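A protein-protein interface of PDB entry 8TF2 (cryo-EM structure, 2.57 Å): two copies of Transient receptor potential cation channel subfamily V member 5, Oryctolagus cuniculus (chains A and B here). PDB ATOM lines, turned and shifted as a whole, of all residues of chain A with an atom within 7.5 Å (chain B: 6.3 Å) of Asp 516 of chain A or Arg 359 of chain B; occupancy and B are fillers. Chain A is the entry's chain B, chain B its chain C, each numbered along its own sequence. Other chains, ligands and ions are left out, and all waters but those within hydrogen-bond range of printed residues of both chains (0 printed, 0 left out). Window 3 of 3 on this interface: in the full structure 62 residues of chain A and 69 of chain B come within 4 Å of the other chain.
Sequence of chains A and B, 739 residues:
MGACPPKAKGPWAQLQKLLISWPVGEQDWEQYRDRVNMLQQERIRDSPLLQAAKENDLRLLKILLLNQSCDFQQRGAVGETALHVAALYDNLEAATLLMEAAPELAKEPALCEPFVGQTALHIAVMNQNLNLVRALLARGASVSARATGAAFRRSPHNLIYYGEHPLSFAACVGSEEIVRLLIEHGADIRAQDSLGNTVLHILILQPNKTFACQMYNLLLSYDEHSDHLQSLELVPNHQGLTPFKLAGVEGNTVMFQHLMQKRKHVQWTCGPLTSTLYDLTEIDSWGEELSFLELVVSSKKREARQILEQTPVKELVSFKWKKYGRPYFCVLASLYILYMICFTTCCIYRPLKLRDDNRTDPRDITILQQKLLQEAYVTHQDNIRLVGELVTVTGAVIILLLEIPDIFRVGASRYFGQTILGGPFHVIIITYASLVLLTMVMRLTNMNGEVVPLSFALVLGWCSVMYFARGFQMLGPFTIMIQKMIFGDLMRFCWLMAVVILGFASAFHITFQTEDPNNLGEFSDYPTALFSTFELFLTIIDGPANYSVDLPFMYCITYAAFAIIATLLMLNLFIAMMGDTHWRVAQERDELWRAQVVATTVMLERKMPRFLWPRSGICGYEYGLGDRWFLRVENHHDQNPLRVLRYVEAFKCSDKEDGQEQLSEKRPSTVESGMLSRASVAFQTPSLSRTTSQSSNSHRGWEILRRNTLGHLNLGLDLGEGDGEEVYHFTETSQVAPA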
ATOM      1  N   PHE A 512       3.563  28.214  -1.201  1.00  0.00           N
ATOM      2  CA  PHE A 512       3.322  29.117  -2.321  1.00  0.00           C
ATOM      3  C   PHE A 512       4.539  29.905  -2.806  1.00  0.00           C
ATOM      4  O   PHE A 512       4.464  30.487  -3.879  1.00  0.00           O
ATOM      5  CB  PHE A 512       2.107  29.993  -2.018  1.00  0.00           C
ATOM      6  CG  PHE A 512       0.844  29.197  -2.229  1.00  0.00           C
ATOM      7  CD1 PHE A 512       0.405  28.944  -3.538  1.00  0.00           C
ATOM      8  CD2 PHE A 512       0.183  28.599  -1.148  1.00  0.00           C
ATOM      9  CE1 PHE A 512      -0.681  28.088  -3.766  1.00  0.00           C
ATOM     10  CE2 PHE A 512      -0.917  27.766  -1.375  1.00  0.00           C
ATOM     11  CZ  PHE A 512      -1.345  27.499  -2.683  1.00  0.00           C
ATOM     12  N   GLN A 513       5.677  29.881  -2.112  1.00  0.00           N
ATOM     13  CA  GLN A 513       6.899  30.584  -2.529  1.00  0.00           C
ATOM     14  C   GLN A 513       7.316  30.301  -3.979  1.00  0.00           C
ATOM     15  O   GLN A 513       7.778  31.197  -4.677  1.00  0.00           O
ATOM     16  CB  GLN A 513       8.058  30.151  -1.627  1.00  0.00           C
ATOM     17  CG  GLN A 513       8.237  30.974  -0.354  1.00  0.00           C
ATOM     18  CD  GLN A 513       9.299  30.365   0.545  1.00  0.00           C
ATOM     19  OE1 GLN A 513       9.506  29.160   0.592  1.00  0.00           O
ATOM     20  NE2 GLN A 513      10.018  31.148   1.297  1.00  0.00           N
ATOM     21  N   THR A 514       7.172  29.061  -4.442  1.00  0.00           N
ATOM     22  CA  THR A 514       7.552  28.636  -5.796  1.00  0.00           C
ATOM     23  C   THR A 514       6.520  28.946  -6.875  1.00  0.00           C
ATOM     24  O   THR A 514       6.828  28.837  -8.055  1.00  0.00           O
ATOM     25  CB  THR A 514       7.905  27.145  -5.815  1.00  0.00           C
ATOM     26  OG1 THR A 514       6.971  26.402  -5.078  1.00  0.00           O
ATOM     27  CG2 THR A 514       9.269  26.889  -5.184  1.00  0.00           C
ATOM     28  N   GLU A 515       5.318  29.373  -6.503  1.00  0.00           N
ATOM     29  CA  GLU A 515       4.174  29.538  -7.390  1.00  0.00           C
ATOM     30  C   GLU A 515       3.921  31.011  -7.734  1.00  0.00           C
ATOM     31  O   GLU A 515       4.296  31.914  -6.996  1.00  0.00           O
ATOM     32  CB  GLU A 515       2.921  28.932  -6.745  1.00  0.00           C
ATOM     33  CG  GLU A 515       3.101  27.550  -6.104  1.00  0.00           C
ATOM     34  CD  GLU A 515       3.885  26.568  -6.982  1.00  0.00           C
ATOM     35  OE1 GLU A 515       3.504  26.358  -8.149  1.00  0.00           O
ATOM     36  OE2 GLU A 515       4.899  26.011  -6.510  1.00  0.00           O
ATOM     37  N   ASP A 516       3.261  31.267  -8.855  1.00  0.00           N
ATOM     38  CA  ASP A 516       2.971  32.601  -9.367  1.00  0.00           C
ATOM     39  C   ASP A 516       1.980  33.369  -8.459  1.00  0.00           C
ATOM     40  O   ASP A 516       0.823  32.951  -8.340  1.00  0.00           O
ATOM     41  CB  ASP A 516       2.454  32.429 -10.801  1.00  0.00           C
ATOM     42  CG  ASP A 516       2.241  33.739 -11.561  1.00  0.00           C
ATOM     43  OD1 ASP A 516       2.193  34.812 -10.922  1.00  0.00           O
ATOM     44  OD2 ASP A 516       2.185  33.685 -12.812  1.00  0.00           O
ATOM     45  N   PRO A 517       2.368  34.502  -7.837  1.00  0.00           N
ATOM     46  CA  PRO A 517       1.508  35.224  -6.903  1.00  0.00           C
ATOM     47  C   PRO A 517       0.206  35.733  -7.518  1.00  0.00           C
ATOM     48  O   PRO A 517      -0.757  35.983  -6.800  1.00  0.00           O
ATOM     49  CB  PRO A 517       2.346  36.402  -6.404  1.00  0.00           C
ATOM     50  CG  PRO A 517       3.781  35.938  -6.594  1.00  0.00           C
ATOM     51  CD  PRO A 517       3.686  35.113  -7.869  1.00  0.00           C
ATOM     52  N   ASN A 518       0.148  35.902  -8.841  1.00  0.00           N
ATOM     53  CA  ASN A 518      -1.036  36.407  -9.527  1.00  0.00           C
ATOM     54  C   ASN A 518      -2.154  35.361  -9.632  1.00  0.00           C
ATOM     55  O   ASN A 518      -3.304  35.725  -9.870  1.00  0.00           O
ATOM     56  CB  ASN A 518      -0.623  36.926 -10.911  1.00  0.00           C
ATOM     57  CG  ASN A 518       0.476  37.977 -10.897  1.00  0.00           C
ATOM     58  OD1 ASN A 518       1.351  37.995 -11.744  1.00  0.00           O
ATOM     59  ND2 ASN A 518       0.484  38.894  -9.958  1.00  0.00           N
ATOM     60  N   ASN A 519      -1.845  34.073  -9.454  1.00  0.00           N
ATOM     61  CA  ASN A 519      -2.833  32.996  -9.505  1.00  0.00           C
ATOM     62  C   ASN A 519      -3.408  32.622  -8.129  1.00  0.00           C
ATOM     63  O   ASN A 519      -4.537  32.142  -8.071  1.00  0.00           O
ATOM     64  CB  ASN A 519      -2.210  31.804 -10.238  1.00  0.00           C
ATOM     65  CG  ASN A 519      -1.881  32.143 -11.681  1.00  0.00           C
ATOM     66  OD1 ASN A 519      -0.738  32.230 -12.078  1.00  0.00           O
ATOM     67  ND2 ASN A 519      -2.868  32.375 -12.511  1.00  0.00           N
ATOM     68  N   LEU A 520      -2.681  32.857  -7.032  1.00  0.00           N
ATOM     69  CA  LEU A 520      -3.171  32.722  -5.655  1.00  0.00           C
ATOM     70  C   LEU A 520      -2.411  33.696  -4.743  1.00  0.00           C
ATOM     71  O   LEU A 520      -1.227  33.517  -4.469  1.00  0.00           O
ATOM     72  CB  LEU A 520      -3.072  31.246  -5.218  1.00  0.00           C
ATOM     73  CG  LEU A 520      -3.832  30.907  -3.917  1.00  0.00           C
ATOM     74  CD1 LEU A 520      -4.213  29.431  -3.943  1.00  0.00           C
ATOM     75  CD2 LEU A 520      -3.012  31.144  -2.650  1.00  0.00           C
ATOM     76  N   GLY A 521      -3.087  34.761  -4.310  1.00  0.00           N
ATOM     77  CA  GLY A 521      -2.461  35.907  -3.648  1.00  0.00           C
ATOM     78  C   GLY A 521      -2.350  35.819  -2.129  1.00  0.00           C
ATOM     79  O   GLY A 521      -1.516  36.508  -1.550  1.00  0.00           O
ATOM     80  N   SER A 524       1.281  35.220  -0.589  1.00  0.00           N
ATOM     81  CA  SER A 524       2.302  35.740  -1.510  1.00  0.00           C
ATOM     82  C   SER A 524       3.517  36.383  -0.829  1.00  0.00           C
ATOM     83  O   SER A 524       4.612  36.344  -1.381  1.00  0.00           O
ATOM     84  CB  SER A 524       1.655  36.722  -2.487  1.00  0.00           C
ATOM     85  OG  SER A 524       0.917  37.727  -1.813  1.00  0.00           O
ATOM     86  N   VAL A 549      -6.117  26.430 -12.486  1.00  0.00           N
ATOM     87  CA  VAL A 549      -4.691  26.086 -12.346  1.00  0.00           C
ATOM     88  C   VAL A 549      -4.481  24.909 -11.395  1.00  0.00           C
ATOM     89  O   VAL A 549      -5.343  24.573 -10.591  1.00  0.00           O
ATOM     90  CB  VAL A 549      -3.841  27.285 -11.879  1.00  0.00           C
ATOM     91  CG1 VAL A 549      -3.939  28.478 -12.828  1.00  0.00           C
ATOM     92  CG2 VAL A 549      -4.177  27.752 -10.467  1.00  0.00           C
ATOM     93  N   ARG B 355      12.868  29.110 -12.251  1.00  0.00           N
ATOM     94  CA  ARG B 355      12.745  27.808 -12.912  1.00  0.00           C
ATOM     95  C   ARG B 355      13.451  27.822 -14.274  1.00  0.00           C
ATOM     96  O   ARG B 355      13.259  28.744 -15.064  1.00  0.00           O
ATOM     97  CB  ARG B 355      11.241  27.532 -13.020  1.00  0.00           C
ATOM     98  CG  ARG B 355      10.865  26.193 -13.649  1.00  0.00           C
ATOM     99  CD  ARG B 355       9.344  26.161 -13.791  1.00  0.00           C
ATOM    100  NE  ARG B 355       8.859  24.939 -14.446  1.00  0.00           N
ATOM    101  CZ  ARG B 355       7.594  24.633 -14.623  1.00  0.00           C
ATOM    102  NH1 ARG B 355       7.245  23.560 -15.250  1.00  0.00           N
ATOM    103  NH2 ARG B 355       6.635  25.380 -14.180  1.00  0.00           N
ATOM    104  N   ASP B 357      13.203  25.144 -16.569  1.00  0.00           N
ATOM    105  CA  ASP B 357      12.083  24.618 -17.354  1.00  0.00           C
ATOM    106  C   ASP B 357      11.035  25.704 -17.713  1.00  0.00           C
ATOM    107  O   ASP B 357      11.006  26.788 -17.130  1.00  0.00           O
ATOM    108  CB  ASP B 357      11.486  23.479 -16.508  1.00  0.00           C
ATOM    109  CG  ASP B 357      10.357  22.700 -17.179  1.00  0.00           C
ATOM    110  OD1 ASP B 357      10.396  22.540 -18.419  1.00  0.00           O
ATOM    111  OD2 ASP B 357       9.440  22.257 -16.449  1.00  0.00           O
ATOM    112  N   ASN B 358      10.139  25.416 -18.660  1.00  0.00           N
ATOM    113  CA  ASN B 358       9.096  26.336 -19.140  1.00  0.00           C
ATOM    114  C   ASN B 358       7.689  25.930 -18.669  1.00  0.00           C
ATOM    115  O   ASN B 358       7.333  24.751 -18.677  1.00  0.00           O
ATOM    116  CB  ASN B 358       9.157  26.421 -20.675  1.00  0.00           C
ATOM    117  CG  ASN B 358      10.407  27.122 -21.169  1.00  0.00           C
ATOM    118  OD1 ASN B 358      10.545  28.331 -21.067  1.00  0.00           O
ATOM    119  ND2 ASN B 358      11.345  26.403 -21.729  1.00  0.00           N
ATOM    120  N   ARG B 359       6.865  26.950 -18.405  1.00  0.00           N
ATOM    121  CA  ARG B 359       5.448  26.688 -18.048  1.00  0.00           C
ATOM    122  C   ARG B 359       4.702  26.544 -19.373  1.00  0.00           C
ATOM    123  O   ARG B 359       4.036  27.512 -19.782  1.00  0.00           O
ATOM    124  CB  ARG B 359       4.887  27.767 -17.118  1.00  0.00           C
ATOM    125  CG  ARG B 359       5.691  28.006 -15.852  1.00  0.00           C
ATOM    126  CD  ARG B 359       5.353  29.384 -15.327  1.00  0.00           C
ATOM    127  NE  ARG B 359       3.929  29.536 -15.079  1.00  0.00           N
ATOM    128  CZ  ARG B 359       3.352  30.680 -14.743  1.00  0.00           C
ATOM    129  NH1 ARG B 359       2.050  30.730 -14.523  1.00  0.00           N
ATOM    130  NH2 ARG B 359       4.077  31.777 -14.632  1.00  0.00           N
ATOM    131  N   THR B 360       4.856  25.410 -20.038  1.00  0.00           N
ATOM    132  CA  THR B 360       4.194  25.049 -21.307  1.00  0.00           C
ATOM    133  C   THR B 360       2.720  24.671 -21.125  1.00  0.00           C
ATOM    134  O   THR B 360       1.898  24.954 -21.994  1.00  0.00           O
ATOM    135  CB  THR B 360       4.935  23.894 -22.000  1.00  0.00           C
ATOM    136  OG1 THR B 360       5.045  22.767 -21.154  1.00  0.00           O
ATOM    137  CG2 THR B 360       6.351  24.296 -22.407  1.00  0.00           C
ATOM    138  N   ASP B 361       2.362  24.054 -19.999  1.00  0.00           N
ATOM    139  CA  ASP B 361       0.973  23.801 -19.603  1.00  0.00           C
ATOM    140  C   ASP B 361       0.326  25.099 -19.077  1.00  0.00           C
ATOM    141  O   ASP B 361       0.858  25.685 -18.134  1.00  0.00           O
ATOM    142  CB  ASP B 361       0.982  22.688 -18.543  1.00  0.00           C
ATOM    143  CG  ASP B 361      -0.392  22.275 -18.010  1.00  0.00           C
ATOM    144  OD1 ASP B 361      -1.401  22.950 -18.294  1.00  0.00           O
ATOM    145  OD2 ASP B 361      -0.452  21.246 -17.304  1.00  0.00           O
ATOM    146  N   PRO B 362      -0.811  25.574 -19.615  1.00  0.00           N
ATOM    147  CA  PRO B 362      -1.465  26.785 -19.119  1.00  0.00           C
ATOM    148  C   PRO B 362      -1.958  26.689 -17.666  1.00  0.00           C
ATOM    149  O   PRO B 362      -2.172  27.722 -17.035  1.00  0.00           O
ATOM    150  CB  PRO B 362      -2.620  27.047 -20.090  1.00  0.00           C
ATOM    151  CG  PRO B 362      -2.935  25.667 -20.653  1.00  0.00           C
ATOM    152  CD  PRO B 362      -1.559  25.017 -20.729  1.00  0.00           C
ATOM    153  N   ASP B 364      -0.115  25.272 -15.212  1.00  0.00           N
ATOM    154  CA  ASP B 364       1.097  25.279 -14.390  1.00  0.00           C
ATOM    155  C   ASP B 364       1.478  26.696 -13.925  1.00  0.00           C
ATOM    156  O   ASP B 364       1.714  27.588 -14.737  1.00  0.00           O
ATOM    157  CB  ASP B 364       2.209  24.613 -15.205  1.00  0.00           C
ATOM    158  CG  ASP B 364       3.560  24.504 -14.505  1.00  0.00           C
ATOM    159  OD1 ASP B 364       3.754  25.026 -13.392  1.00  0.00           O
ATOM    160  OD2 ASP B 364       4.479  23.904 -15.097  1.00  0.00           O
ATOM    161  N   ILE B 365       1.553  26.895 -12.609  1.00  0.00           N
ATOM    162  CA  ILE B 365       1.880  28.172 -11.960  1.00  0.00           C
ATOM    163  C   ILE B 365       3.248  28.191 -11.270  1.00  0.00           C
ATOM    164  O   ILE B 365       3.589  29.188 -10.648  1.00  0.00           O
ATOM    165  CB  ILE B 365       0.741  28.624 -11.019  1.00  0.00           C
ATOM    166  CG1 ILE B 365       0.441  27.606  -9.902  1.00  0.00           C
ATOM    167  CG2 ILE B 365      -0.503  28.940 -11.854  1.00  0.00           C
ATOM    168  CD1 ILE B 365      -0.444  28.163  -8.784  1.00  0.00           C
ATOM    169  N   THR B 366       4.063  27.145 -11.368  1.00  0.00           N
ATOM    170  CA  THR B 366       5.368  27.121 -10.706  1.00  0.00           C
ATOM    171  C   THR B 366       6.380  27.980 -11.461  1.00  0.00           C
ATOM    172  O   THR B 366       6.708  27.692 -12.609  1.00  0.00           O
ATOM    173  CB  THR B 366       5.870  25.691 -10.545  1.00  0.00           C
ATOM    174  OG1 THR B 366       4.946  24.949  -9.798  1.00  0.00           O
ATOM    175  CG2 THR B 366       7.198  25.610  -9.809  1.00  0.00           C
ATOM    176  N   ILE B 367       6.900  29.023 -10.819  1.00  0.00           N
ATOM    177  CA  ILE B 367       7.856  29.986 -11.389  1.00  0.00           C
ATOM    178  C   ILE B 367       9.254  29.915 -10.762  1.00  0.00           C
ATOM    179  O   ILE B 367      10.233  30.232 -11.432  1.00  0.00           O
ATOM    180  CB  ILE B 367       7.306  31.424 -11.296  1.00  0.00           C
ATOM    181  CG1 ILE B 367       6.896  31.825  -9.870  1.00  0.00           C
ATOM    182  CG2 ILE B 367       6.144  31.603 -12.271  1.00  0.00           C
ATOM    183  CD1 ILE B 367       6.778  33.330  -9.663  1.00  0.00           C
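No position is printed for both chains. Of the 11 pairs that touch across the chains among the printed residues, none has its exchanged pair printed and touching as well.
OD2 of Asp 516 of chain A is in salt-bridge range of NH2 of Arg 359 of chain B (3.2 Å). O of Thr 514 of chain A sits at hydrogen-bond distance from N of Ile 367 of chain B (2.8 Å). The backbone carbonyl oxygen (O) of Ile 365 of chain B sits at hydrogen-bond distance from the backbone NH (N) of Asp 516 of chain A (2.8 Å). OE1 of Glu 515 of chain A is in hydrogen-bond range of OG1 of Thr 366 of chain B (2.6 Å).
Asp 516 of chain A touches just these residues of chain B: Arg 359, Ile 365 and Ile 367. Of the printed residues of chain B, Pro 517 of chain A touches Ile 367. Of the printed residues of chain B, Asn 519 of chain A touches Ile 365. Of the printed residues of chain A, Arg 359 of chain B touches Asp 516 (3.2 Å). Printed residues of chain A within 4 Å of Thr 366 of chain B: Thr 514 (3.5 Å) and Glu 515 (2.6 Å). Printed residues of chain A within 4 Å of Ile 367 of chain B: Thr 514, Glu 515, Asp 516 and Pro 517. The nearest residue of chain B that does not touch Asp 516 of chain A is Thr 366 of chain B (4.9 Å). The nearest printed residue of chain A that does not touch Arg 359 of chain B is Asn 519 of chain A (4.0001 Å). The nearest printed residue of chain B that does not touch Glu 515 of chain A is Asp 364 of chain B (5.4 Å).
Of the 12 printed residues of chain A, 6 touch a printed residue of chain B. Printed residues of chain B that touch a printed residue of chain A: Arg 359, Ile 365, Thr 366 and Ile 367. Hydrophobic or aromatic side chains of chain B that line the printed part of chain A: Ile 365 and Ile 367. Along chain B the printed residues that touch a printed residue of chain A span positions 359 to 367. Among the printed residues, Asp or Glu carboxylates within 4 Å of a Lys or Arg side-chain nitrogen of the other chain: Asp 516 of chain A with Arg 359 of chain B (3.2 Å).
OD2 of Asp 516 of chain A lies close to OD1 of Asn 519 of chain A, 3.3 Å away. The side-chain carboxylate (OE2) of Glu 515 of chain A is in hydrogen-bond range of the side-chain hydroxyl (OG1) of Thr 514 of chain A. The guanidinium group of Arg 355 of chain B lies within hydrogen-bond range of the backbone carbonyl oxygen of Thr 366 of chain B (2.8 Å). NE of Arg 359 of chain B lies within hydrogen-bond range of O of Asp 364 of chain B (3.0 Å). OD1 of Asp 364 of chain B sits at hydrogen-bond distance from N of Thr 366 of chain B, at 2.9 Å. The side-chain carboxylate of Asp 516 of chain A is in hydrogen-bond range of the backbone NH of Asn 518 of chain A (3.1 Å).
Thr 366 of chain B touches Thr 514 of chain A. Glu 515 of chain A touches Ile 365 of chain B. Ile 367 of chain B touches Glu 515 of chain A. CG1 of Ile 367 of chain B touches N of Asp 516 of chain A, at 3.8 Å. Pro 517 of chain A touches Ile 367 of chain B (CD to CD1, 3.99 Å). Asn 519 of chain A touches Ile 365 of chain B (OD1 to CG2, 3.3 Å). Val 549 of chain A touches Ile 365 of chain B (CG1 to CG2, 3.6 Å).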
